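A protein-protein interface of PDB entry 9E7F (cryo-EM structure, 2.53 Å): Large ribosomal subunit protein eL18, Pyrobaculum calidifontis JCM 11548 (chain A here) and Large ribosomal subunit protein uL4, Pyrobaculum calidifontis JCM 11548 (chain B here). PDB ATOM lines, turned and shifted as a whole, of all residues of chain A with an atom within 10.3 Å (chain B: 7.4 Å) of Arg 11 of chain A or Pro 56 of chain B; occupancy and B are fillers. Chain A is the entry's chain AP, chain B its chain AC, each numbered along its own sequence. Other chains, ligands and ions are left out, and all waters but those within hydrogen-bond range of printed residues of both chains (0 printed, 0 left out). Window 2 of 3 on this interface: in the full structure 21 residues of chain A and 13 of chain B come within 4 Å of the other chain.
OD2 of Asp 57 of chain B is in salt-bridge range of NH2 of Arg 55 of chain B (3.7 Å).
The backbone NH (N) of Gln 12 of chain A lies within hydrogen-bond range of the side-chain amide oxygen (OD1) of Asn 10 of chain A (3.0 Å).
The side-chain hydroxyl of Ser 145 of chain B lies within hydrogen-bond range of the backbone carbonyl oxygen of Pro 53 of chain B (2.9 Å).
The backbone NH (N) of Arg 55 of chain B is in hydrogen-bond range of the side-chain hydroxyl (OG) of Ser 145 of chain B (3.0 Å).
NE of Arg 55 of chain B is in hydrogen-bond range of OD1 of Asn 10 of chain A, 3.2 Å away.
Thr 9 of chain A touches Asp 57 of chain B.
Asn 10 of chain A touches Asp 57 of chain B.
Arg 11 of chain A touches Pro 56 of chain B (NH1 to CG, 3.6 Å).
Gln 12 of chain A touches Pro 53 of chain B.
No residue of chain A comes within 4 Å of Ile 59 of chain B.
Printed residues of chain A within 4 Å of Asp 57 of chain B: Thr 9 and Asn 10.
Printed residues of chain B within 4 Å of Thr 9 of chain A: Asp 57 (3.5 Å).
Of the printed residues of chain A, Pro 53 of chain B touches Gln 12 (3.99 Å).
The nearest printed residue of chain A that does not touch Pro 56 of chain B is Asn 10 of chain A (7.4 Å).
The nearest printed residue of chain A that does not touch Pro 53 of chain B is Asn 10 of chain A (7.0 Å).
Hydrophobic or aromatic side chains of chain B that line the printed part of chain A: Pro 53 and Pro 56.
Of the 15 printed residues of chain A, 4 touch a printed residue of chain B.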
ATOM      1  N   GLY A   7      27.583 -11.870 -22.150  1.00  0.00           N
ATOM      2  CA  GLY A   7      28.274 -12.932 -21.468  1.00  0.00           C
ATOM      3  C   GLY A   7      27.305 -13.696 -20.596  1.00  0.00           C
ATOM      4  O   GLY A   7      26.176 -13.257 -20.366  1.00  0.00           O
ATOM      5  N   PRO A   8      27.726 -14.857 -20.099  1.00  0.00           N
ATOM      6  CA  PRO A   8      26.816 -15.701 -19.313  1.00  0.00           C
ATOM      7  C   PRO A   8      26.409 -15.047 -18.002  1.00  0.00           C
ATOM      8  O   PRO A   8      27.187 -14.322 -17.379  1.00  0.00           O
ATOM      9  CB  PRO A   8      27.628 -16.977 -19.068  1.00  0.00           C
ATOM     10  CG  PRO A   8      28.891 -16.837 -19.816  1.00  0.00           C
ATOM     11  CD  PRO A   8      29.069 -15.435 -20.238  1.00  0.00           C
ATOM     12  N   THR A   9      25.168 -15.305 -17.592  1.00  0.00           N
ATOM     13  CA  THR A   9      24.660 -14.846 -16.308  1.00  0.00           C
ATOM     14  C   THR A   9      24.888 -15.860 -15.203  1.00  0.00           C
ATOM     15  O   THR A   9      24.917 -15.489 -14.026  1.00  0.00           O
ATOM     16  CB  THR A   9      23.165 -14.539 -16.408  1.00  0.00           C
ATOM     17  OG1 THR A   9      22.918 -13.761 -17.582  1.00  0.00           O
ATOM     18  CG2 THR A   9      22.689 -13.772 -15.192  1.00  0.00           C
ATOM     19  N   ASN A  10      25.031 -17.132 -15.564  1.00  0.00           N
ATOM     20  CA  ASN A  10      25.368 -18.173 -14.606  1.00  0.00           C
ATOM     21  C   ASN A  10      26.730 -17.891 -13.985  1.00  0.00           C
ATOM     22  O   ASN A  10      27.702 -17.625 -14.694  1.00  0.00           O
ATOM     23  CB  ASN A  10      25.369 -19.526 -15.318  1.00  0.00           C
ATOM     24  CG  ASN A  10      25.450 -20.696 -14.371  1.00  0.00           C
ATOM     25  OD1 ASN A  10      25.611 -20.532 -13.167  1.00  0.00           O
ATOM     26  ND2 ASN A  10      25.340 -21.896 -14.917  1.00  0.00           N
ATOM     27  N   ARG A  11      26.797 -17.946 -12.656  1.00  0.00           N
ATOM     28  CA  ARG A  11      28.066 -17.732 -11.975  1.00  0.00           C
ATOM     29  C   ARG A  11      28.974 -18.941 -12.078  1.00  0.00           C
ATOM     30  O   ARG A  11      30.195 -18.804 -11.976  1.00  0.00           O
ATOM     31  CB  ARG A  11      27.835 -17.392 -10.507  1.00  0.00           C
ATOM     32  CG  ARG A  11      27.857 -15.916 -10.207  1.00  0.00           C
ATOM     33  CD  ARG A  11      27.059 -15.626  -8.959  1.00  0.00           C
ATOM     34  NE  ARG A  11      27.029 -14.205  -8.646  1.00  0.00           N
ATOM     35  CZ  ARG A  11      26.451 -13.693  -7.569  1.00  0.00           C
ATOM     36  NH1 ARG A  11      25.850 -14.460  -6.677  1.00  0.00           N
ATOM     37  NH2 ARG A  11      26.473 -12.376  -7.386  1.00  0.00           N
ATOM     38  N   GLN A  12      28.400 -20.131 -12.239  1.00  0.00           N
ATOM     39  CA  GLN A  12      29.222 -21.316 -12.429  1.00  0.00           C
ATOM     40  C   GLN A  12      29.999 -21.232 -13.733  1.00  0.00           C
ATOM     41  O   GLN A  12      31.174 -21.609 -13.794  1.00  0.00           O
ATOM     42  CB  GLN A  12      28.345 -22.563 -12.397  1.00  0.00           C
ATOM     43  CG  GLN A  12      27.829 -22.891 -11.012  1.00  0.00           C
ATOM     44  CD  GLN A  12      28.839 -23.667 -10.191  1.00  0.00           C
ATOM     45  OE1 GLN A  12      29.784 -23.096  -9.649  1.00  0.00           O
ATOM     46  NE2 GLN A  12      28.646 -24.976 -10.100  1.00  0.00           N
ATOM     47  N   LEU A  13      29.359 -20.732 -14.786  1.00  0.00           N
ATOM     48  CA  LEU A  13      30.054 -20.524 -16.045  1.00  0.00           C
ATOM     49  C   LEU A  13      31.036 -19.368 -15.946  1.00  0.00           C
ATOM     50  O   LEU A  13      32.088 -19.388 -16.594  1.00  0.00           O
ATOM     51  CB  LEU A  13      29.041 -20.280 -17.156  1.00  0.00           C
ATOM     52  CG  LEU A  13      28.066 -21.438 -17.351  1.00  0.00           C
ATOM     53  CD1 LEU A  13      26.857 -21.025 -18.171  1.00  0.00           C
ATOM     54  CD2 LEU A  13      28.785 -22.607 -17.991  1.00  0.00           C
ATOM     55  N   ARG A  14      30.706 -18.344 -15.159  1.00  0.00           N
ATOM     56  CA  ARG A  14      31.615 -17.217 -14.987  1.00  0.00           C
ATOM     57  C   ARG A  14      32.895 -17.640 -14.282  1.00  0.00           C
ATOM     58  O   ARG A  14      33.988 -17.188 -14.639  1.00  0.00           O
ATOM     59  CB  ARG A  14      30.923 -16.098 -14.212  1.00  0.00           C
ATOM     60  CG  ARG A  14      29.803 -15.426 -14.970  1.00  0.00           C
ATOM     61  CD  ARG A  14      29.267 -14.220 -14.226  1.00  0.00           C
ATOM     62  NE  ARG A  14      29.997 -13.001 -14.551  1.00  0.00           N
ATOM     63  CZ  ARG A  14      29.708 -12.206 -15.571  1.00  0.00           C
ATOM     64  NH1 ARG A  14      28.713 -12.475 -16.397  1.00  0.00           N
ATOM     65  NH2 ARG A  14      30.441 -11.116 -15.773  1.00  0.00           N
ATOM     66  N   MET A  15      32.783 -18.497 -13.268  1.00  0.00           N
ATOM     67  CA  MET A  15      33.965 -18.949 -12.544  1.00  0.00           C
ATOM     68  C   MET A  15      34.809 -19.890 -13.390  1.00  0.00           C
ATOM     69  O   MET A  15      36.042 -19.852 -13.324  1.00  0.00           O
ATOM     70  CB  MET A  15      33.551 -19.622 -11.239  1.00  0.00           C
ATOM     71  CG  MET A  15      33.285 -18.658 -10.103  1.00  0.00           C
ATOM     72  SD  MET A  15      34.393 -17.240 -10.098  1.00  0.00           S
ATOM     73  CE  MET A  15      33.258 -15.937 -10.543  1.00  0.00           C
ATOM     74  N   LEU A  16      34.165 -20.755 -14.175  1.00  0.00           N
ATOM     75  CA  LEU A  16      34.914 -21.659 -15.041  1.00  0.00           C
ATOM     76  C   LEU A  16      35.659 -20.890 -16.125  1.00  0.00           C
ATOM     77  O   LEU A  16      36.780 -21.251 -16.493  1.00  0.00           O
ATOM     78  CB  LEU A  16      33.973 -22.695 -15.651  1.00  0.00           C
ATOM     79  CG  LEU A  16      34.554 -23.590 -16.748  1.00  0.00           C
ATOM     80  CD1 LEU A  16      35.838 -24.260 -16.293  1.00  0.00           C
ATOM     81  CD2 LEU A  16      33.533 -24.622 -17.178  1.00  0.00           C
ATOM     82  N   ILE A  17      35.049 -19.827 -16.646  1.00  0.00           N
ATOM     83  CA  ILE A  17      35.734 -18.959 -17.597  1.00  0.00           C
ATOM     84  C   ILE A  17      36.917 -18.268 -16.934  1.00  0.00           C
ATOM     85  O   ILE A  17      37.990 -18.131 -17.528  1.00  0.00           O
ATOM     86  CB  ILE A  17      34.746 -17.940 -18.189  1.00  0.00           C
ATOM     87  CG1 ILE A  17      33.783 -18.627 -19.155  1.00  0.00           C
ATOM     88  CG2 ILE A  17      35.492 -16.828 -18.873  1.00  0.00           C
ATOM     89  CD1 ILE A  17      32.443 -17.935 -19.273  1.00  0.00           C
ATOM     90  N   ARG A  18      36.730 -17.799 -15.700  1.00  0.00           N
ATOM     91  CA  ARG A  18      37.837 -17.228 -14.942  1.00  0.00           C
ATOM     92  C   ARG A  18      38.909 -18.273 -14.665  1.00  0.00           C
ATOM     93  O   ARG A  18      40.105 -17.967 -14.689  1.00  0.00           O
ATOM     94  CB  ARG A  18      37.317 -16.635 -13.633  1.00  0.00           C
ATOM     95  CG  ARG A  18      38.391 -16.079 -12.734  1.00  0.00           C
ATOM     96  CD  ARG A  18      39.066 -14.916 -13.400  1.00  0.00           C
ATOM     97  NE  ARG A  18      40.115 -14.334 -12.577  1.00  0.00           N
ATOM     98  CZ  ARG A  18      41.254 -13.857 -13.059  1.00  0.00           C
ATOM     99  NH1 ARG A  18      41.526 -13.899 -14.352  1.00  0.00           N
ATOM    100  NH2 ARG A  18      42.146 -13.338 -12.221  1.00  0.00           N
ATOM    101  N   PHE A  19      38.491 -19.511 -14.386  1.00  0.00           N
ATOM    102  CA  PHE A  19      39.430 -20.582 -14.069  1.00  0.00           C
ATOM    103  C   PHE A  19      40.336 -20.887 -15.250  1.00  0.00           C
ATOM    104  O   PHE A  19      41.546 -21.068 -15.086  1.00  0.00           O
ATOM    105  CB  PHE A  19      38.655 -21.834 -13.645  1.00  0.00           C
ATOM    106  CG  PHE A  19      39.523 -23.037 -13.379  1.00  0.00           C
ATOM    107  CD1 PHE A  19      39.728 -24.006 -14.353  1.00  0.00           C
ATOM    108  CD2 PHE A  19      40.113 -23.213 -12.144  1.00  0.00           C
ATOM    109  CE1 PHE A  19      40.522 -25.094 -14.107  1.00  0.00           C
ATOM    110  CE2 PHE A  19      40.897 -24.307 -11.893  1.00  0.00           C
ATOM    111  CZ  PHE A  19      41.107 -25.248 -12.878  1.00  0.00           C
ATOM    112  N   VAL A  39      33.864 -21.200 -24.634  1.00  0.00           N
ATOM    113  CA  VAL A  39      32.854 -21.400 -23.602  1.00  0.00           C
ATOM    114  C   VAL A  39      32.067 -20.122 -23.358  1.00  0.00           C
ATOM    115  O   VAL A  39      30.878 -20.169 -23.029  1.00  0.00           O
ATOM    116  CB  VAL A  39      33.514 -21.915 -22.309  1.00  0.00           C
ATOM    117  CG1 VAL A  39      32.551 -21.838 -21.154  1.00  0.00           C
ATOM    118  CG2 VAL A  39      34.002 -23.335 -22.499  1.00  0.00           C
ATOM    119  N   ARG A  46      26.220 -21.390 -28.634  1.00  0.00           N
ATOM    120  CA  ARG A  46      27.065 -22.228 -27.797  1.00  0.00           C
ATOM    121  C   ARG A  46      27.272 -23.597 -28.426  1.00  0.00           C
ATOM    122  O   ARG A  46      26.357 -24.175 -29.015  1.00  0.00           O
ATOM    123  CB  ARG A  46      26.456 -22.382 -26.409  1.00  0.00           C
ATOM    124  CG  ARG A  46      27.177 -21.586 -25.354  1.00  0.00           C
ATOM    125  CD  ARG A  46      26.413 -21.569 -24.058  1.00  0.00           C
ATOM    126  NE  ARG A  46      26.646 -20.320 -23.349  1.00  0.00           N
ATOM    127  CZ  ARG A  46      25.781 -19.762 -22.520  1.00  0.00           C
ATOM    128  NH1 ARG A  46      24.626 -20.338 -22.241  1.00  0.00           N
ATOM    129  NH2 ARG A  46      26.083 -18.599 -21.954  1.00  0.00           N
ATOM    130  N   PRO B  53      24.071 -26.267  -6.439  1.00  0.00           N
ATOM    131  CA  PRO B  53      24.741 -24.973  -6.274  1.00  0.00           C
ATOM    132  C   PRO B  53      23.724 -23.850  -6.173  1.00  0.00           C
ATOM    133  O   PRO B  53      22.694 -23.861  -6.847  1.00  0.00           O
ATOM    134  CB  PRO B  53      25.589 -24.851  -7.542  1.00  0.00           C
ATOM    135  CG  PRO B  53      24.913 -25.723  -8.527  1.00  0.00           C
ATOM    136  CD  PRO B  53      24.331 -26.860  -7.759  1.00  0.00           C
ATOM    137  N   VAL B  54      24.015 -22.880  -5.317  1.00  0.00           N
ATOM    138  CA  VAL B  54      23.103 -21.763  -5.107  1.00  0.00           C
ATOM    139  C   VAL B  54      23.250 -20.799  -6.277  1.00  0.00           C
ATOM    140  O   VAL B  54      24.326 -20.237  -6.502  1.00  0.00           O
ATOM    141  CB  VAL B  54      23.381 -21.069  -3.768  1.00  0.00           C
ATOM    142  CG1 VAL B  54      22.226 -20.168  -3.391  1.00  0.00           C
ATOM    143  CG2 VAL B  54      23.632 -22.099  -2.693  1.00  0.00           C
ATOM    144  N   ARG B  55      22.167 -20.616  -7.031  1.00  0.00           N
ATOM    145  CA  ARG B  55      22.163 -19.818  -8.255  1.00  0.00           C
ATOM    146  C   ARG B  55      21.160 -18.690  -8.077  1.00  0.00           C
ATOM    147  O   ARG B  55      19.954 -18.871  -8.317  1.00  0.00           O
ATOM    148  CB  ARG B  55      21.836 -20.685  -9.464  1.00  0.00           C
ATOM    149  CG  ARG B  55      22.928 -21.682  -9.765  1.00  0.00           C
ATOM    150  CD  ARG B  55      22.815 -22.234 -11.155  1.00  0.00           C
ATOM    151  NE  ARG B  55      22.600 -21.193 -12.148  1.00  0.00           N
ATOM    152  CZ  ARG B  55      22.177 -21.426 -13.381  1.00  0.00           C
ATOM    153  NH1 ARG B  55      21.933 -22.654 -13.803  1.00  0.00           N
ATOM    154  NH2 ARG B  55      21.992 -20.403 -14.208  1.00  0.00           N
ATOM    155  N   PRO B  56      21.610 -17.523  -7.612  1.00  0.00           N
ATOM    156  CA  PRO B  56      20.677 -16.426  -7.331  1.00  0.00           C
ATOM    157  C   PRO B  56      19.936 -15.905  -8.543  1.00  0.00           C
ATOM    158  O   PRO B  56      18.797 -15.460  -8.392  1.00  0.00           O
ATOM    159  CB  PRO B  56      21.586 -15.352  -6.723  1.00  0.00           C
ATOM    160  CG  PRO B  56      22.733 -16.099  -6.180  1.00  0.00           C
ATOM    161  CD  PRO B  56      22.962 -17.233  -7.118  1.00  0.00           C
ATOM    162  N   ASP B  57      20.529 -15.936  -9.740  1.00  0.00           N
ATOM    163  CA  ASP B  57      19.809 -15.446 -10.912  1.00  0.00           C
ATOM    164  C   ASP B  57      18.660 -16.379 -11.286  1.00  0.00           C
ATOM    165  O   ASP B  57      17.561 -15.920 -11.625  1.00  0.00           O
ATOM    166  CB  ASP B  57      20.777 -15.244 -12.082  1.00  0.00           C
ATOM    167  CG  ASP B  57      21.433 -16.529 -12.539  1.00  0.00           C
ATOM    168  OD1 ASP B  57      21.875 -17.314 -11.677  1.00  0.00           O
ATOM    169  OD2 ASP B  57      21.496 -16.759 -13.763  1.00  0.00           O
ATOM    170  N   LEU B  58      18.883 -17.690 -11.196  1.00  0.00           N
ATOM    171  CA  LEU B  58      17.814 -18.647 -11.435  1.00  0.00           C
ATOM    172  C   LEU B  58      16.750 -18.542 -10.355  1.00  0.00           C
ATOM    173  O   LEU B  58      15.551 -18.650 -10.637  1.00  0.00           O
ATOM    174  CB  LEU B  58      18.397 -20.055 -11.498  1.00  0.00           C
ATOM    175  CG  LEU B  58      17.480 -21.239 -11.748  1.00  0.00           C
ATOM    176  CD1 LEU B  58      16.818 -21.118 -13.096  1.00  0.00           C
ATOM    177  CD2 LEU B  58      18.296 -22.502 -11.669  1.00  0.00           C
ATOM    178  N   ILE B  59      17.175 -18.320  -9.111  1.00  0.00           N
ATOM    179  CA  ILE B  59      16.231 -18.134  -8.015  1.00  0.00           C
ATOM    180  C   ILE B  59      15.388 -16.889  -8.244  1.00  0.00           C
ATOM    181  O   ILE B  59      14.175 -16.897  -8.021  1.00  0.00           O
ATOM    182  CB  ILE B  59      16.986 -18.067  -6.677  1.00  0.00           C
ATOM    183  CG1 ILE B  59      17.458 -19.458  -6.270  1.00  0.00           C
ATOM    184  CG2 ILE B  59      16.117 -17.444  -5.607  1.00  0.00           C
ATOM    185  CD1 ILE B  59      18.591 -19.442  -5.289  1.00  0.00           C
ATOM    186  N   ARG B  60      16.019 -15.802  -8.694  1.00  0.00           N
ATOM    187  CA  ARG B  60      15.305 -14.558  -8.953  1.00  0.00           C
ATOM    188  C   ARG B  60      14.289 -14.734 -10.070  1.00  0.00           C
ATOM    189  O   ARG B  60      13.145 -14.273  -9.962  1.00  0.00           O
ATOM    190  CB  ARG B  60      16.306 -13.454  -9.300  1.00  0.00           C
ATOM    191  CG  ARG B  60      15.684 -12.092  -9.543  1.00  0.00           C
ATOM    192  CD  ARG B  60      16.594 -11.184 -10.346  1.00  0.00           C
ATOM    193  NE  ARG B  60      17.824 -10.849  -9.639  1.00  0.00           N
ATOM    194  CZ  ARG B  60      18.780 -10.074 -10.131  1.00  0.00           C
ATOM    195  NH1 ARG B  60      18.685  -9.539 -11.335  1.00  0.00           N
ATOM    196  NH2 ARG B  60      19.860  -9.828  -9.395  1.00  0.00           N
ATOM    197  N   ARG B  61      14.687 -15.416 -11.148  1.00  0.00           N
ATOM    198  CA  ARG B  61      13.771 -15.663 -12.258  1.00  0.00           C
ATOM    199  C   ARG B  61      12.583 -16.513 -11.822  1.00  0.00           C
ATOM    200  O   ARG B  61      11.434 -16.214 -12.162  1.00  0.00           O
ATOM    201  CB  ARG B  61      14.511 -16.338 -13.407  1.00  0.00           C
ATOM    202  CG  ARG B  61      13.788 -16.213 -14.718  1.00  0.00           C
ATOM    203  CD  ARG B  61      13.778 -17.507 -15.499  1.00  0.00           C
ATOM    204  NE  ARG B  61      13.193 -17.307 -16.819  1.00  0.00           N
ATOM    205  CZ  ARG B  61      13.588 -17.925 -17.921  1.00  0.00           C
ATOM    206  NH1 ARG B  61      14.573 -18.804 -17.905  1.00  0.00           N
ATOM    207  NH2 ARG B  61      12.981 -17.650 -19.069  1.00  0.00           N
ATOM    208  N   ALA B  62      12.837 -17.573 -11.057  1.00  0.00           N
ATOM    209  CA  ALA B  62      11.744 -18.445 -10.652  1.00  0.00           C
ATOM    210  C   ALA B  62      10.845 -17.772  -9.621  1.00  0.00           C
ATOM    211  O   ALA B  62       9.643 -18.046  -9.570  1.00  0.00           O
ATOM    212  CB  ALA B  62      12.297 -19.760 -10.121  1.00  0.00           C
ATOM    213  N   SER B 145      17.600 -25.348  -5.829  1.00  0.00           N
ATOM    214  CA  SER B 145      18.672 -24.391  -5.584  1.00  0.00           C
ATOM    215  C   SER B 145      18.380 -23.531  -4.362  1.00  0.00           C
ATOM    216  O   SER B 145      19.261 -23.296  -3.530  1.00  0.00           O
ATOM    217  CB  SER B 145      18.876 -23.517  -6.817  1.00  0.00           C
ATOM    218  OG  SER B 145      20.043 -22.733  -6.692  1.00  0.00           O
ATOM    219  N   TRP B 155      24.307 -17.375   3.290  1.00  0.00           N
ATOM    220  CA  TRP B 155      23.161 -16.889   2.531  1.00  0.00           C
ATOM    221  C   TRP B 155      22.057 -16.395   3.451  1.00  0.00           C
ATOM    222  O   TRP B 155      21.452 -15.346   3.200  1.00  0.00           O
ATOM    223  CB  TRP B 155      22.630 -17.989   1.615  1.00  0.00           C
ATOM    224  CG  TRP B 155      23.526 -18.325   0.473  1.00  0.00           C
ATOM    225  CD1 TRP B 155      24.256 -19.458   0.323  1.00  0.00           C
ATOM    226  CD2 TRP B 155      23.775 -17.530  -0.692  1.00  0.00           C
ATOM    227  NE1 TRP B 155      24.952 -19.423  -0.855  1.00  0.00           N
ATOM    228  CE2 TRP B 155      24.675 -18.247  -1.499  1.00  0.00           C
ATOM    229  CE3 TRP B 155      23.328 -16.280  -1.128  1.00  0.00           C
ATOM    230  CZ2 TRP B 155      25.140 -17.759  -2.717  1.00  0.00           C
ATOM    231  CZ3 TRP B 155      23.790 -15.798  -2.338  1.00  0.00           C
ATOM    232  CH2 TRP B 155      24.685 -16.537  -3.118  1.00  0.00           C
ATOM    233  N   ALA B 261      12.545 -17.833  -1.256  1.00  0.00           N
ATOM    234  CA  ALA B 261      13.402 -16.702  -1.613  1.00  0.00           C
ATOM    235  C   ALA B 261      12.562 -15.438  -1.693  1.00  0.00           C
ATOM    236  O   ALA B 261      12.282 -14.924  -2.780  1.00  0.00           O
ATOM    237  CB  ALA B 261      14.119 -16.963  -2.934  1.00  0.00           C
ATOM    238  N   GLY B 264      13.212 -12.363  -4.084  1.00  0.00           N
ATOM    239  CA  GLY B 264      14.032 -12.904  -5.142  1.00  0.00           C
ATOM    240  C   GLY B 264      15.444 -13.249  -4.736  1.00  0.00           C
ATOM    241  O   GLY B 264      16.222 -13.699  -5.584  1.00  0.00           O
ATOM    242  N   VAL B 265      15.797 -13.065  -3.470  1.00  0.00           N
ATOM    243  CA  VAL B 265      17.143 -13.326  -2.979  1.00  0.00           C
ATOM    244  C   VAL B 265      17.140 -14.652  -2.231  1.00  0.00           C
ATOM    245  O   VAL B 265      16.234 -14.908  -1.426  1.00  0.00           O
ATOM    246  CB  VAL B 265      17.632 -12.180  -2.082  1.00  0.00           C
ATOM    247  CG1 VAL B 265      18.953 -12.536  -1.438  1.00  0.00           C
ATOM    248  CG2 VAL B 265      17.759 -10.907  -2.889  1.00  0.00           C
ATOM    249  N   PRO B 266      18.119 -15.518  -2.457  1.00  0.00           N
ATOM    250  CA  PRO B 266      18.121 -16.826  -1.803  1.00  0.00           C
ATOM    251  C   PRO B 266      18.475 -16.741  -0.325  1.00  0.00           C
ATOM    252  O   PRO B 266      19.083 -15.785   0.153  1.00  0.00           O
ATOM    253  CB  PRO B 266      19.190 -17.613  -2.570  1.00  0.00           C
ATOM    254  CG  PRO B 266      19.694 -16.710  -3.641  1.00  0.00           C
ATOM    255  CD  PRO B 266      19.297 -15.325  -3.312  1.00  0.00           C
